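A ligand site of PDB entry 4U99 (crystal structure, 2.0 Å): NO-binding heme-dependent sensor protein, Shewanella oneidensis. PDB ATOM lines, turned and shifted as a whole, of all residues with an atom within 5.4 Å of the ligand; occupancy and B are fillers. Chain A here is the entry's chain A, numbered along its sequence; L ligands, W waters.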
ATOM      1  N   MET A   1      -2.189  18.130   8.953  1.00  0.00           N
ATOM      2  CA  MET A   1      -1.371  19.259   9.480  1.00  0.00           C
ATOM      3  C   MET A   1      -0.666  19.986   8.331  1.00  0.00           C
ATOM      4  O   MET A   1       0.177  19.396   7.652  1.00  0.00           O
ATOM      5  CB  MET A   1      -0.338  18.742  10.492  1.00  0.00           C
ATOM      6  CG  MET A   1       0.417  19.841  11.227  1.00  0.00           C
ATOM      7  SD  MET A   1      -0.611  20.750  12.412  1.00  0.00           S
ATOM      8  CE  MET A   1      -1.015  19.470  13.595  1.00  0.00           C
ATOM      9  N   LYS A   2      -1.012  21.253   8.124  1.00  0.00           N
ATOM     10  CA  LYS A   2      -0.491  22.000   6.984  1.00  0.00           C
ATOM     11  C   LYS A   2       0.989  22.318   7.121  1.00  0.00           C
ATOM     12  O   LYS A   2       1.499  22.562   8.217  1.00  0.00           O
ATOM     13  CB  LYS A   2      -1.277  23.304   6.794  1.00  0.00           C
ATOM     14  CG  LYS A   2      -2.714  23.093   6.303  1.00  0.00           C
ATOM     15  CD  LYS A   2      -2.747  22.405   4.952  1.00  0.00           C
ATOM     16  CE  LYS A   2      -4.163  22.259   4.428  1.00  0.00           C
ATOM     17  NZ  LYS A   2      -4.205  21.539   3.134  1.00  0.00           N
ATOM     18  N   ILE A   4       2.700  24.823   6.600  1.00  0.00           N
ATOM     19  CA  ILE A   4       3.037  26.093   7.210  1.00  0.00           C
ATOM     20  C   ILE A   4       3.390  25.933   8.698  1.00  0.00           C
ATOM     21  O   ILE A   4       4.294  26.594   9.198  1.00  0.00           O
ATOM     22  CB  ILE A   4       1.906  27.125   7.078  1.00  0.00           C
ATOM     23  CG1 ILE A   4       2.332  28.440   7.722  1.00  0.00           C
ATOM     24  CG2 ILE A   4       0.605  26.602   7.701  1.00  0.00           C
ATOM     25  CD1 ILE A   4       1.453  29.585   7.384  1.00  0.00           C
ATOM     26  N   ILE A   5       2.683  25.042   9.381  1.00  0.00           N
ATOM     27  CA  ILE A   5       2.968  24.769  10.794  1.00  0.00           C
ATOM     28  C   ILE A   5       4.380  24.202  10.921  1.00  0.00           C
ATOM     29  O   ILE A   5       5.160  24.633  11.768  1.00  0.00           O
ATOM     30  CB  ILE A   5       1.948  23.791  11.407  1.00  0.00           C
ATOM     31  CG1 ILE A   5       0.517  24.285  11.166  1.00  0.00           C
ATOM     32  CG2 ILE A   5       2.197  23.612  12.905  1.00  0.00           C
ATOM     33  CD1 ILE A   5       0.225  25.682  11.704  1.00  0.00           C
ATOM     34  N   SER A  41      -1.159  19.452   3.030  1.00  0.00           N
ATOM     35  CA  SER A  41      -1.424  18.710   4.264  1.00  0.00           C
ATOM     36  C   SER A  41      -0.425  17.577   4.462  1.00  0.00           C
ATOM     37  O   SER A  41      -0.056  16.893   3.508  1.00  0.00           O
ATOM     38  CB  SER A  41      -2.843  18.146   4.245  1.00  0.00           C
ATOM     39  OG  SER A  41      -3.808  19.151   4.465  1.00  0.00           O
ATOM     40  N   PHE A  74       2.258  32.236  16.620  1.00  0.00           N
ATOM     41  CA  PHE A  74       1.339  33.324  16.278  1.00  0.00           C
ATOM     42  C   PHE A  74       2.014  34.345  15.374  1.00  0.00           C
ATOM     43  O   PHE A  74       1.415  34.802  14.410  1.00  0.00           O
ATOM     44  CB  PHE A  74       0.790  34.047  17.509  1.00  0.00           C
ATOM     45  CG  PHE A  74      -0.199  35.120  17.147  1.00  0.00           C
ATOM     46  CD1 PHE A  74       0.242  36.404  16.829  1.00  0.00           C
ATOM     47  CD2 PHE A  74      -1.549  34.834  17.054  1.00  0.00           C
ATOM     48  CE1 PHE A  74      -0.657  37.385  16.459  1.00  0.00           C
ATOM     49  CE2 PHE A  74      -2.448  35.815  16.683  1.00  0.00           C
ATOM     50  CZ  PHE A  74      -2.002  37.091  16.386  1.00  0.00           C
ATOM     51  N   LEU A  77       2.415  32.984  11.881  1.00  0.00           N
ATOM     52  CA  LEU A  77       1.158  33.050  11.148  1.00  0.00           C
ATOM     53  C   LEU A  77       0.785  34.485  10.798  1.00  0.00           C
ATOM     54  O   LEU A  77       0.313  34.753   9.700  1.00  0.00           O
ATOM     55  CB  LEU A  77       0.034  32.388  11.951  1.00  0.00           C
ATOM     56  CG  LEU A  77       0.139  30.879  12.122  1.00  0.00           C
ATOM     57  CD1 LEU A  77      -0.902  30.371  13.118  1.00  0.00           C
ATOM     58  CD2 LEU A  77      -0.017  30.176  10.787  1.00  0.00           C
ATOM     59  N   ALA A  78       0.996  35.400  11.735  1.00  0.00           N
ATOM     60  CA  ALA A  78       0.645  36.798  11.518  1.00  0.00           C
ATOM     61  C   ALA A  78       1.489  37.413  10.402  1.00  0.00           C
ATOM     62  O   ALA A  78       1.005  38.259   9.665  1.00  0.00           O
ATOM     63  CB  ALA A  78       0.822  37.605  12.807  1.00  0.00           C
ATOM     64  N   HIS A  81       0.260  35.756   7.095  1.00  0.00           N
ATOM     65  CA  HIS A  81      -1.120  36.146   6.787  1.00  0.00           C
ATOM     66  C   HIS A  81      -1.446  37.487   7.422  1.00  0.00           C
ATOM     67  O   HIS A  81      -2.361  37.602   8.225  1.00  0.00           O
ATOM     68  CB  HIS A  81      -2.105  35.102   7.291  1.00  0.00           C
ATOM     69  CG  HIS A  81      -1.984  33.769   6.629  1.00  0.00           C
ATOM     70  ND1 HIS A  81      -2.301  33.569   5.297  1.00  0.00           N
ATOM     71  CD2 HIS A  81      -1.596  32.570   7.111  1.00  0.00           C
ATOM     72  CE1 HIS A  81      -2.096  32.299   4.991  1.00  0.00           C
ATOM     73  NE2 HIS A  81      -1.676  31.670   6.073  1.00  0.00           N
ATOM     74  N   VAL A  84      -4.980  38.895   7.337  1.00  0.00           N
ATOM     75  CA  VAL A  84      -5.965  38.309   8.230  1.00  0.00           C
ATOM     76  C   VAL A  84      -5.896  38.966   9.615  1.00  0.00           C
ATOM     77  O   VAL A  84      -6.913  39.368  10.172  1.00  0.00           O
ATOM     78  CB  VAL A  84      -5.762  36.778   8.385  1.00  0.00           C
ATOM     79  CG1 VAL A  84      -6.780  36.194   9.350  1.00  0.00           C
ATOM     80  CG2 VAL A  84      -5.893  36.090   7.021  1.00  0.00           C
ATOM     81  N   VAL A  85      -4.687  39.085  10.158  1.00  0.00           N
ATOM     82  CA  VAL A  85      -4.518  39.655  11.491  1.00  0.00           C
ATOM     83  C   VAL A  85      -4.793  41.162  11.503  1.00  0.00           C
ATOM     84  O   VAL A  85      -5.262  41.700  12.509  1.00  0.00           O
ATOM     85  CB  VAL A  85      -3.095  39.376  12.018  1.00  0.00           C
ATOM     86  CG1 VAL A  85      -2.885  40.008  13.396  1.00  0.00           C
ATOM     87  CG2 VAL A  85      -2.864  37.876  12.110  1.00  0.00           C
ATOM     88  N   LEU A  94      -9.591  40.129  18.221  1.00  0.00           N
ATOM     89  CA  LEU A  94      -8.993  38.995  17.522  1.00  0.00           C
ATOM     90  C   LEU A  94      -9.436  37.663  18.126  1.00  0.00           C
ATOM     91  O   LEU A  94      -9.793  36.736  17.388  1.00  0.00           O
ATOM     92  CB  LEU A  94      -7.459  39.083  17.548  1.00  0.00           C
ATOM     93  CG  LEU A  94      -6.738  38.005  16.736  1.00  0.00           C
ATOM     94  CD1 LEU A  94      -5.505  38.566  16.036  1.00  0.00           C
ATOM     95  CD2 LEU A  94      -6.355  36.821  17.614  1.00  0.00           C
ATOM     96  N   VAL A  95      -9.403  37.558  19.450  1.00  0.00           N
ATOM     97  CA  VAL A  95      -9.797  36.309  20.116  1.00  0.00           C
ATOM     98  C   VAL A  95     -11.240  35.965  19.784  1.00  0.00           C
ATOM     99  O   VAL A  95     -11.566  34.818  19.462  1.00  0.00           O
ATOM    100  CB  VAL A  95      -9.610  36.393  21.642  1.00  0.00           C
ATOM    101  CG1 VAL A  95     -10.173  35.154  22.334  1.00  0.00           C
ATOM    102  CG2 VAL A  95      -8.143  36.565  21.992  1.00  0.00           C
ATOM    103  N   ILE A  98     -11.502  34.463  16.231  1.00  0.00           N
ATOM    104  CA  ILE A  98     -10.677  33.320  15.832  1.00  0.00           C
ATOM    105  C   ILE A  98     -11.471  32.343  14.973  1.00  0.00           C
ATOM    106  O   ILE A  98     -11.012  31.931  13.907  1.00  0.00           O
ATOM    107  CB  ILE A  98     -10.112  32.561  17.051  1.00  0.00           C
ATOM    108  CG1 ILE A  98      -9.101  33.442  17.794  1.00  0.00           C
ATOM    109  CG2 ILE A  98      -9.424  31.266  16.610  1.00  0.00           C
ATOM    110  CD1 ILE A  98      -8.738  32.907  19.197  1.00  0.00           C
ATOM    111  N   ILE A 102     -10.937  34.417  11.464  1.00  0.00           N
ATOM    112  CA  ILE A 102      -9.613  33.898  11.132  1.00  0.00           C
ATOM    113  C   ILE A 102      -9.676  32.499  10.517  1.00  0.00           C
ATOM    114  O   ILE A 102      -9.260  32.296   9.384  1.00  0.00           O
ATOM    115  CB  ILE A 102      -8.694  33.883  12.363  1.00  0.00           C
ATOM    116  CG1 ILE A 102      -8.491  35.315  12.862  1.00  0.00           C
ATOM    117  CG2 ILE A 102      -7.354  33.232  12.038  1.00  0.00           C
ATOM    118  CD1 ILE A 102      -7.663  35.443  14.108  1.00  0.00           C
ATOM    119  N   HIS A 103     -10.211  31.535  11.252  1.00  0.00           N
ATOM    120  CA  HIS A 103     -10.204  30.154  10.772  1.00  0.00           C
ATOM    121  C   HIS A 103     -11.215  29.968   9.647  1.00  0.00           C
ATOM    122  O   HIS A 103     -11.089  29.034   8.845  1.00  0.00           O
ATOM    123  CB  HIS A 103     -10.474  29.193  11.943  1.00  0.00           C
ATOM    124  CG  HIS A 103      -9.277  28.988  12.830  1.00  0.00           C
ATOM    125  ND1 HIS A 103      -9.376  28.433  14.083  1.00  0.00           N
ATOM    126  CD2 HIS A 103      -7.967  29.255  12.633  1.00  0.00           C
ATOM    127  CE1 HIS A 103      -8.171  28.370  14.623  1.00  0.00           C
ATOM    128  NE2 HIS A 103      -7.302  28.861  13.771  1.00  0.00           N
ATOM    129  N   VAL A 106      -9.031  30.787   6.829  1.00  0.00           N
ATOM    130  CA  VAL A 106      -8.104  29.686   6.628  1.00  0.00           C
ATOM    131  C   VAL A 106      -8.739  28.610   5.752  1.00  0.00           C
ATOM    132  O   VAL A 106      -8.051  27.981   4.942  1.00  0.00           O
ATOM    133  CB  VAL A 106      -7.650  29.085   7.979  1.00  0.00           C
ATOM    134  CG1 VAL A 106      -6.828  27.824   7.779  1.00  0.00           C
ATOM    135  CG2 VAL A 106      -6.840  30.113   8.756  1.00  0.00           C
ATOM    136  N   TYR A 110      -6.707  27.686   2.427  1.00  0.00           N
ATOM    137  CA  TYR A 110      -6.158  26.340   2.385  1.00  0.00           C
ATOM    138  C   TYR A 110      -7.220  25.321   1.980  1.00  0.00           C
ATOM    139  O   TYR A 110      -8.397  25.479   2.301  1.00  0.00           O
ATOM    140  CB  TYR A 110      -5.579  25.940   3.746  1.00  0.00           C
ATOM    141  CG  TYR A 110      -4.384  26.749   4.203  1.00  0.00           C
ATOM    142  CD1 TYR A 110      -4.553  27.921   4.924  1.00  0.00           C
ATOM    143  CD2 TYR A 110      -3.097  26.330   3.915  1.00  0.00           C
ATOM    144  CE1 TYR A 110      -3.457  28.666   5.353  1.00  0.00           C
ATOM    145  CE2 TYR A 110      -1.996  27.063   4.333  1.00  0.00           C
ATOM    146  CZ  TYR A 110      -2.187  28.237   5.049  1.00  0.00           C
ATOM    147  OH  TYR A 110      -1.095  28.981   5.468  1.00  0.00           O
ATOM    148  N   GLU A 112      -9.108  22.178   2.700  1.00  0.00           N
ATOM    149  CA  GLU A 112      -9.502  21.269   3.775  1.00  0.00           C
ATOM    150  C   GLU A 112      -8.509  21.229   4.946  1.00  0.00           C
ATOM    151  O   GLU A 112      -7.915  20.188   5.221  1.00  0.00           O
ATOM    152  CB  GLU A 112      -9.688  19.849   3.219  1.00  0.00           C
ATOM    153  CG  GLU A 112     -10.821  19.760   2.213  1.00  0.00           C
ATOM    154  CD  GLU A 112     -11.038  18.356   1.685  1.00  0.00           C
ATOM    155  OE1 GLU A 112     -10.347  17.417   2.152  1.00  0.00           O
ATOM    156  OE2 GLU A 112     -11.892  18.190   0.783  1.00  0.00           O
ATOM    157  N   PRO A 113      -8.338  22.362   5.626  1.00  0.00           N
ATOM    158  CA  PRO A 113      -7.473  22.418   6.815  1.00  0.00           C
ATOM    159  C   PRO A 113      -8.083  21.621   7.963  1.00  0.00           C
ATOM    160  O   PRO A 113      -9.290  21.413   7.969  1.00  0.00           O
ATOM    161  CB  PRO A 113      -7.417  23.906   7.132  1.00  0.00           C
ATOM    162  CG  PRO A 113      -8.711  24.430   6.651  1.00  0.00           C
ATOM    163  CD  PRO A 113      -9.012  23.650   5.395  1.00  0.00           C
ATOM    164  N   SER A 114      -7.254  21.198   8.911  1.00  0.00           N
ATOM    165  CA  SER A 114      -7.727  20.525  10.114  1.00  0.00           C
ATOM    166  C   SER A 114      -7.645  21.489  11.281  1.00  0.00           C
ATOM    167  O   SER A 114      -6.570  21.717  11.854  1.00  0.00           O
ATOM    168  CB  SER A 114      -6.903  19.266  10.383  1.00  0.00           C
ATOM    169  OG  SER A 114      -7.167  18.281   9.405  1.00  0.00           O
ATOM    170  N   LEU A 115      -8.791  22.071  11.620  1.00  0.00           N
ATOM    171  CA  LEU A 115      -8.866  23.169  12.570  1.00  0.00           C
ATOM    172  C   LEU A 115      -9.675  22.788  13.813  1.00  0.00           C
ATOM    173  O   LEU A 115     -10.553  21.929  13.739  1.00  0.00           O
ATOM    174  CB  LEU A 115      -9.496  24.394  11.915  1.00  0.00           C
ATOM    175  CG  LEU A 115      -8.671  25.030  10.793  1.00  0.00           C
ATOM    176  CD1 LEU A 115      -9.560  25.891   9.908  1.00  0.00           C
ATOM    177  CD2 LEU A 115      -7.534  25.840  11.382  1.00  0.00           C
ATOM    178  N   PRO A 116      -9.393  23.435  14.951  1.00  0.00           N
ATOM    179  CA  PRO A 116     -10.177  23.168  16.156  1.00  0.00           C
ATOM    180  C   PRO A 116     -11.536  23.847  16.088  1.00  0.00           C
ATOM    181  O   PRO A 116     -11.742  24.700  15.219  1.00  0.00           O
ATOM    182  CB  PRO A 116      -9.321  23.783  17.268  1.00  0.00           C
ATOM    183  CG  PRO A 116      -8.661  24.942  16.586  1.00  0.00           C
ATOM    184  CD  PRO A 116      -8.395  24.500  15.171  1.00  0.00           C
ATOM    185  N   ILE A 118     -13.662  26.463  18.118  1.00  0.00           N
ATOM    186  CA  ILE A 118     -13.455  27.480  19.141  1.00  0.00           C
ATOM    187  C   ILE A 118     -14.661  28.396  19.249  1.00  0.00           C
ATOM    188  O   ILE A 118     -15.287  28.740  18.240  1.00  0.00           O
ATOM    189  CB  ILE A 118     -12.173  28.294  18.843  1.00  0.00           C
ATOM    190  CG1 ILE A 118     -10.942  27.397  19.008  1.00  0.00           C
ATOM    191  CG2 ILE A 118     -12.078  29.514  19.776  1.00  0.00           C
ATOM    192  CD1 ILE A 118      -9.620  28.060  18.659  1.00  0.00           C
ATOM    193  N   LEU A 130     -12.867  31.200  26.554  1.00  0.00           N
ATOM    194  CA  LEU A 130     -12.603  30.589  25.258  1.00  0.00           C
ATOM    195  C   LEU A 130     -12.718  29.064  25.357  1.00  0.00           C
ATOM    196  O   LEU A 130     -11.897  28.416  26.003  1.00  0.00           O
ATOM    197  CB  LEU A 130     -11.230  30.984  24.730  1.00  0.00           C
ATOM    198  CG  LEU A 130     -11.011  30.740  23.239  1.00  0.00           C
ATOM    199  CD1 LEU A 130     -11.838  31.713  22.411  1.00  0.00           C
ATOM    200  CD2 LEU A 130      -9.540  30.859  22.863  1.00  0.00           C
ATOM    201  N   TYR A 132     -12.462  25.454  23.745  1.00  0.00           N
ATOM    202  CA  TYR A 132     -11.659  24.808  22.716  1.00  0.00           C
ATOM    203  C   TYR A 132     -11.995  23.326  22.635  1.00  0.00           C
ATOM    204  O   TYR A 132     -12.130  22.658  23.658  1.00  0.00           O
ATOM    205  CB  TYR A 132     -10.163  24.982  23.017  1.00  0.00           C
ATOM    206  CG  TYR A 132      -9.242  24.123  22.182  1.00  0.00           C
ATOM    207  CD1 TYR A 132      -8.921  22.830  22.576  1.00  0.00           C
ATOM    208  CD2 TYR A 132      -8.668  24.609  21.018  1.00  0.00           C
ATOM    209  CE1 TYR A 132      -8.082  22.031  21.832  1.00  0.00           C
ATOM    210  CE2 TYR A 132      -7.820  23.828  20.259  1.00  0.00           C
ATOM    211  CZ  TYR A 132      -7.525  22.539  20.671  1.00  0.00           C
ATOM    212  OH  TYR A 132      -6.685  21.750  19.925  1.00  0.00           O
ATOM    213  N   SER A 134     -10.997  19.785  19.992  1.00  0.00           N
ATOM    214  CA  SER A 134     -10.298  19.237  18.839  1.00  0.00           C
ATOM    215  C   SER A 134      -9.812  17.811  19.103  1.00  0.00           C
ATOM    216  O   SER A 134      -9.325  17.520  20.189  1.00  0.00           O
ATOM    217  CB  SER A 134      -9.113  20.113  18.459  1.00  0.00           C
ATOM    218  OG  SER A 134      -8.265  19.453  17.523  1.00  0.00           O
ATOM    219  N   ARG A 136      -7.228  16.614  18.054  1.00  0.00           N
ATOM    220  CA  ARG A 136      -5.774  16.709  18.164  1.00  0.00           C
ATOM    221  C   ARG A 136      -5.339  17.179  19.566  1.00  0.00           C
ATOM    222  O   ARG A 136      -4.180  17.040  19.937  1.00  0.00           O
ATOM    223  CB  ARG A 136      -5.227  17.654  17.095  1.00  0.00           C
ATOM    224  CG  ARG A 136      -5.305  17.056  15.686  1.00  0.00           C
ATOM    225  CD  ARG A 136      -5.236  18.129  14.606  1.00  0.00           C
ATOM    226  NE  ARG A 136      -6.442  18.958  14.565  1.00  0.00           N
ATOM    227  CZ  ARG A 136      -7.584  18.578  14.014  1.00  0.00           C
ATOM    228  NH1 ARG A 136      -7.697  17.383  13.460  1.00  0.00           N
ATOM    229  NH2 ARG A 136      -8.629  19.396  14.033  1.00  0.00           N
ATOM    230  N   LEU A 138      -4.782  20.069  21.102  1.00  0.00           N
ATOM    231  CA  LEU A 138      -3.645  20.993  21.097  1.00  0.00           C
ATOM    232  C   LEU A 138      -3.975  22.268  21.865  1.00  0.00           C
ATOM    233  O   LEU A 138      -3.594  23.366  21.455  1.00  0.00           O
ATOM    234  CB  LEU A 138      -3.265  21.324  19.647  1.00  0.00           C
ATOM    235  CG  LEU A 138      -2.568  20.194  18.888  1.00  0.00           C
ATOM    236  CD1 LEU A 138      -2.505  20.503  17.394  1.00  0.00           C
ATOM    237  CD2 LEU A 138      -1.170  19.972  19.448  1.00  0.00           C
ATOM    238  N   CYS A 141      -1.118  24.478  22.629  1.00  0.00           N
ATOM    239  CA  CYS A 141      -0.715  25.288  21.486  1.00  0.00           C
ATOM    240  C   CYS A 141      -1.613  26.516  21.418  1.00  0.00           C
ATOM    241  O   CYS A 141      -1.146  27.613  21.171  1.00  0.00           O
ATOM    242  CB  CYS A 141      -0.791  24.498  20.177  1.00  0.00           C
ATOM    243  SG  CYS A 141      -0.070  25.364  18.751  1.00  0.00           S
ATOM    244  N   ALA A 142      -2.910  26.314  21.668  1.00  0.00           N
ATOM    245  CA  ALA A 142      -3.856  27.419  21.717  1.00  0.00           C
ATOM    246  C   ALA A 142      -3.472  28.441  22.773  1.00  0.00           C
ATOM    247  O   ALA A 142      -3.516  29.651  22.516  1.00  0.00           O
ATOM    248  CB  ALA A 142      -5.269  26.905  21.964  1.00  0.00           C
ATOM    249  N   LEU A 145      -0.604  30.395  21.480  1.00  0.00           N
ATOM    250  CA  LEU A 145      -1.063  31.294  20.428  1.00  0.00           C
ATOM    251  C   LEU A 145      -1.719  32.541  21.010  1.00  0.00           C
ATOM    252  O   LEU A 145      -1.558  33.638  20.485  1.00  0.00           O
ATOM    253  CB  LEU A 145      -2.025  30.567  19.481  1.00  0.00           C
ATOM    254  CG  LEU A 145      -1.309  29.724  18.420  1.00  0.00           C
ATOM    255  CD1 LEU A 145      -2.223  28.642  17.864  1.00  0.00           C
ATOM    256  CD2 LEU A 145      -0.798  30.605  17.293  1.00  0.00           C
ATOM    257  N   LEU A 146      -2.455  32.378  22.109  1.00  0.00           N
ATOM    258  CA  LEU A 146      -3.111  33.501  22.753  1.00  0.00           C
ATOM    259  C   LEU A 146      -2.084  34.447  23.371  1.00  0.00           C
ATOM    260  O   LEU A 146      -2.227  35.675  23.276  1.00  0.00           O
ATOM    261  CB  LEU A 146      -4.099  33.016  23.815  1.00  0.00           C
ATOM    262  CG  LEU A 146      -5.341  32.340  23.234  1.00  0.00           C
ATOM    263  CD1 LEU A 146      -6.055  31.544  24.308  1.00  0.00           C
ATOM    264  CD2 LEU A 146      -6.270  33.367  22.618  1.00  0.00           C
ATOM    265  N   ALA A 149      -0.685  36.324  20.520  1.00  0.00           N
ATOM    266  CA  ALA A 149      -1.608  37.374  20.109  1.00  0.00           C
ATOM    267  C   ALA A 149      -1.525  38.576  21.047  1.00  0.00           C
ATOM    268  O   ALA A 149      -1.564  39.723  20.606  1.00  0.00           O
ATOM    269  CB  ALA A 149      -3.022  36.836  20.056  1.00  0.00           C
HETATM  270  C1  LIG L   1      -4.508  25.485  13.493  1.00  0.00           C
HETATM  271  C2  LIG L   1      -5.800  28.084  17.363  1.00  0.00           C
HETATM  272  C3  LIG L   1      -4.626  32.185  15.086  1.00  0.00           C
HETATM  273  C4  LIG L   1      -4.337  29.660  10.952  1.00  0.00           C
HETATM  274  C5  LIG L   1      -4.763  25.843  14.797  1.00  0.00           C
HETATM  275  C6  LIG L   1      -4.602  24.997  15.960  1.00  0.00           C
HETATM  276  C7  LIG L   1      -4.954  25.723  17.031  1.00  0.00           C
HETATM  277  C8  LIG L   1      -5.358  27.039  16.586  1.00  0.00           C
HETATM  278  C9  LIG L   1      -4.935  25.263  18.515  1.00  0.00           C
HETATM  279  C10 LIG L   1      -4.090  23.537  15.949  1.00  0.00           C
HETATM  280  C11 LIG L   1      -5.119  22.581  15.332  1.00  0.00           C
HETATM  281  C12 LIG L   1      -6.116  22.070  16.336  1.00  0.00           C
HETATM  282  O1  LIG L   1      -6.959  21.205  15.971  1.00  0.00           O
HETATM  283  O2  LIG L   1      -6.099  22.498  17.526  1.00  0.00           O
HETATM  284  C13 LIG L   1      -5.550  29.417  17.127  1.00  0.00           C
HETATM  285  C14 LIG L   1      -5.621  30.487  18.100  1.00  0.00           C
HETATM  286  C15 LIG L   1      -5.293  31.636  17.471  1.00  0.00           C
HETATM  287  C16 LIG L   1      -5.006  31.306  16.082  1.00  0.00           C
HETATM  288  C17 LIG L   1      -6.023  30.252  19.579  1.00  0.00           C
HETATM  289  C18 LIG L   1      -5.193  33.083  18.008  1.00  0.00           C
HETATM  290  C19 LIG L   1      -5.062  33.379  19.301  1.00  0.00           C
HETATM  291  C20 LIG L   1      -4.446  31.863  13.758  1.00  0.00           C
HETATM  292  C21 LIG L   1      -4.084  32.789  12.711  1.00  0.00           C
HETATM  293  C22 LIG L   1      -3.990  32.082  11.566  1.00  0.00           C
HETATM  294  C23 LIG L   1      -4.306  30.700  11.856  1.00  0.00           C
HETATM  295  C24 LIG L   1      -3.840  34.297  12.942  1.00  0.00           C
HETATM  296  C25 LIG L   1      -3.656  32.572  10.136  1.00  0.00           C
HETATM  297  C26 LIG L   1      -4.047  33.778   9.717  1.00  0.00           C
HETATM  298  C27 LIG L   1      -4.204  28.315  11.258  1.00  0.00           C
HETATM  299  C28 LIG L   1      -3.709  27.291  10.359  1.00  0.00           C
HETATM  300  C29 LIG L   1      -3.771  25.992  11.155  1.00  0.00           C
HETATM  301  C30 LIG L   1      -4.286  26.356  12.459  1.00  0.00           C
HETATM  302  C31 LIG L   1      -3.226  27.459   8.904  1.00  0.00           C
HETATM  303  C32 LIG L   1      -3.346  24.589  10.684  1.00  0.00           C
HETATM  304  C33 LIG L   1      -4.527  23.859  10.049  1.00  0.00           C
HETATM  305  C34 LIG L   1      -4.045  22.544   9.512  1.00  0.00           C
HETATM  306  O3  LIG L   1      -2.891  22.158   9.833  1.00  0.00           O
HETATM  307  O4  LIG L   1      -4.806  21.881   8.773  1.00  0.00           O
HETATM  308  N1  LIG L   1      -5.240  27.071  15.204  1.00  0.00           N
HETATM  309  N2  LIG L   1      -5.172  29.948  15.911  1.00  0.00           N
HETATM  310  N3  LIG L   1      -4.578  30.609  13.203  1.00  0.00           N
HETATM  311  N4  LIG L   1      -4.536  27.729  12.476  1.00  0.00           N
HETATM  312 FE1  LIG L   1      -5.127  28.844  14.166  1.00  0.00          FE
HETATM  313  O   HOH W   1      -4.112  20.552  12.204  1.00  0.00           O
HETATM  314  O   HOH W   2      -4.055  19.626   7.426  1.00  0.00           O
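A ring nitrogen (NE2) of His 103 is bound to an iron atom (FE1) of the ligand (2.2 Å).
O4 of the ligand is in hydrogen-bond range of N of Ser 114.
The side-chain hydroxyl of Tyr 132 lies within hydrogen-bond range of an oxygen (O2) of the ligand (2.6 Å).
OG of Ser 134 sits at hydrogen-bond distance from O1 of the ligand (2.7 Å).
N of Lys 2 sits at hydrogen-bond distance from O3 of the ligand, 2.7 Å away.
The guanidinium group (NE) of Arg 136 is in salt-bridge range of an oxygen (O1) of the ligand (2.7 Å).
SD of Met 1 lies close to O3 of the ligand (3.7 Å).
An oxygen (O1) of the ligand lies close to the backbone nitrogen of Pro 116, 3.5 Å away.
Residues that only touch the ligand: Ile 5 (3.9 Å), Leu 77 (3.6 Å), His 81 (3.4 Å), Val 84 (3.7 Å), Val 85 (3.8 Å), Leu 94 (3.9 Å), Ile 98 (3.7 Å), Ile 102 (3.4 Å), Val 106 (3.4 Å), Tyr 110 (3.8 Å), Pro 113 (3.4 Å), Leu 115 (3.5 Å), Leu 138 (3.7 Å), Ala 142 (3.8 Å), Leu 145 (3.5 Å) and Leu 146 (3.5 Å).
Hydrophobic or aromatic side chains within 4 Å of the ligand: Met 1, Ile 5, Leu 77, His 81, Val 84, Val 85, Leu 94, Ile 98, Ile 102, His 103, Val 106, Tyr 110, Pro 113, Leu 115, Pro 116, Tyr 132, Leu 138, Ala 142, Leu 145 and Leu 146.
The backbone NH of His 103 is in hydrogen-bond range of the backbone carbonyl oxygen of Ile 98 (2.8 Å).
OH of Tyr 132 lies within hydrogen-bond range of N of Leu 138 (2.8 Å).
The side-chain hydroxyl (OG) of Ser 134 sits close to the backbone NH (N) of Arg 136.
The side-chain amino group of Lys 2 sits at hydrogen-bond distance from the side-chain hydroxyl of Ser 41 (2.8 Å).
The guanidinium group (NH2) of Arg 136 is in hydrogen-bond range of the backbone carbonyl oxygen (O) of Leu 115.
A ring nitrogen (NE2) of His 81 lies within hydrogen-bond range of the side-chain hydroxyl of Tyr 110, 2.8 Å away.
Water W2 lies within hydrogen-bond range of O4 of the ligand (2.7 Å), N of Met 1 (2.8 Å) and OG of Ser 41 (3.0 Å).
Water W1 lies within hydrogen-bond range of O of Ser 114 (2.7 Å), O3 of the ligand (3.1 Å) and SD of Met 1 (3.5 Å).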
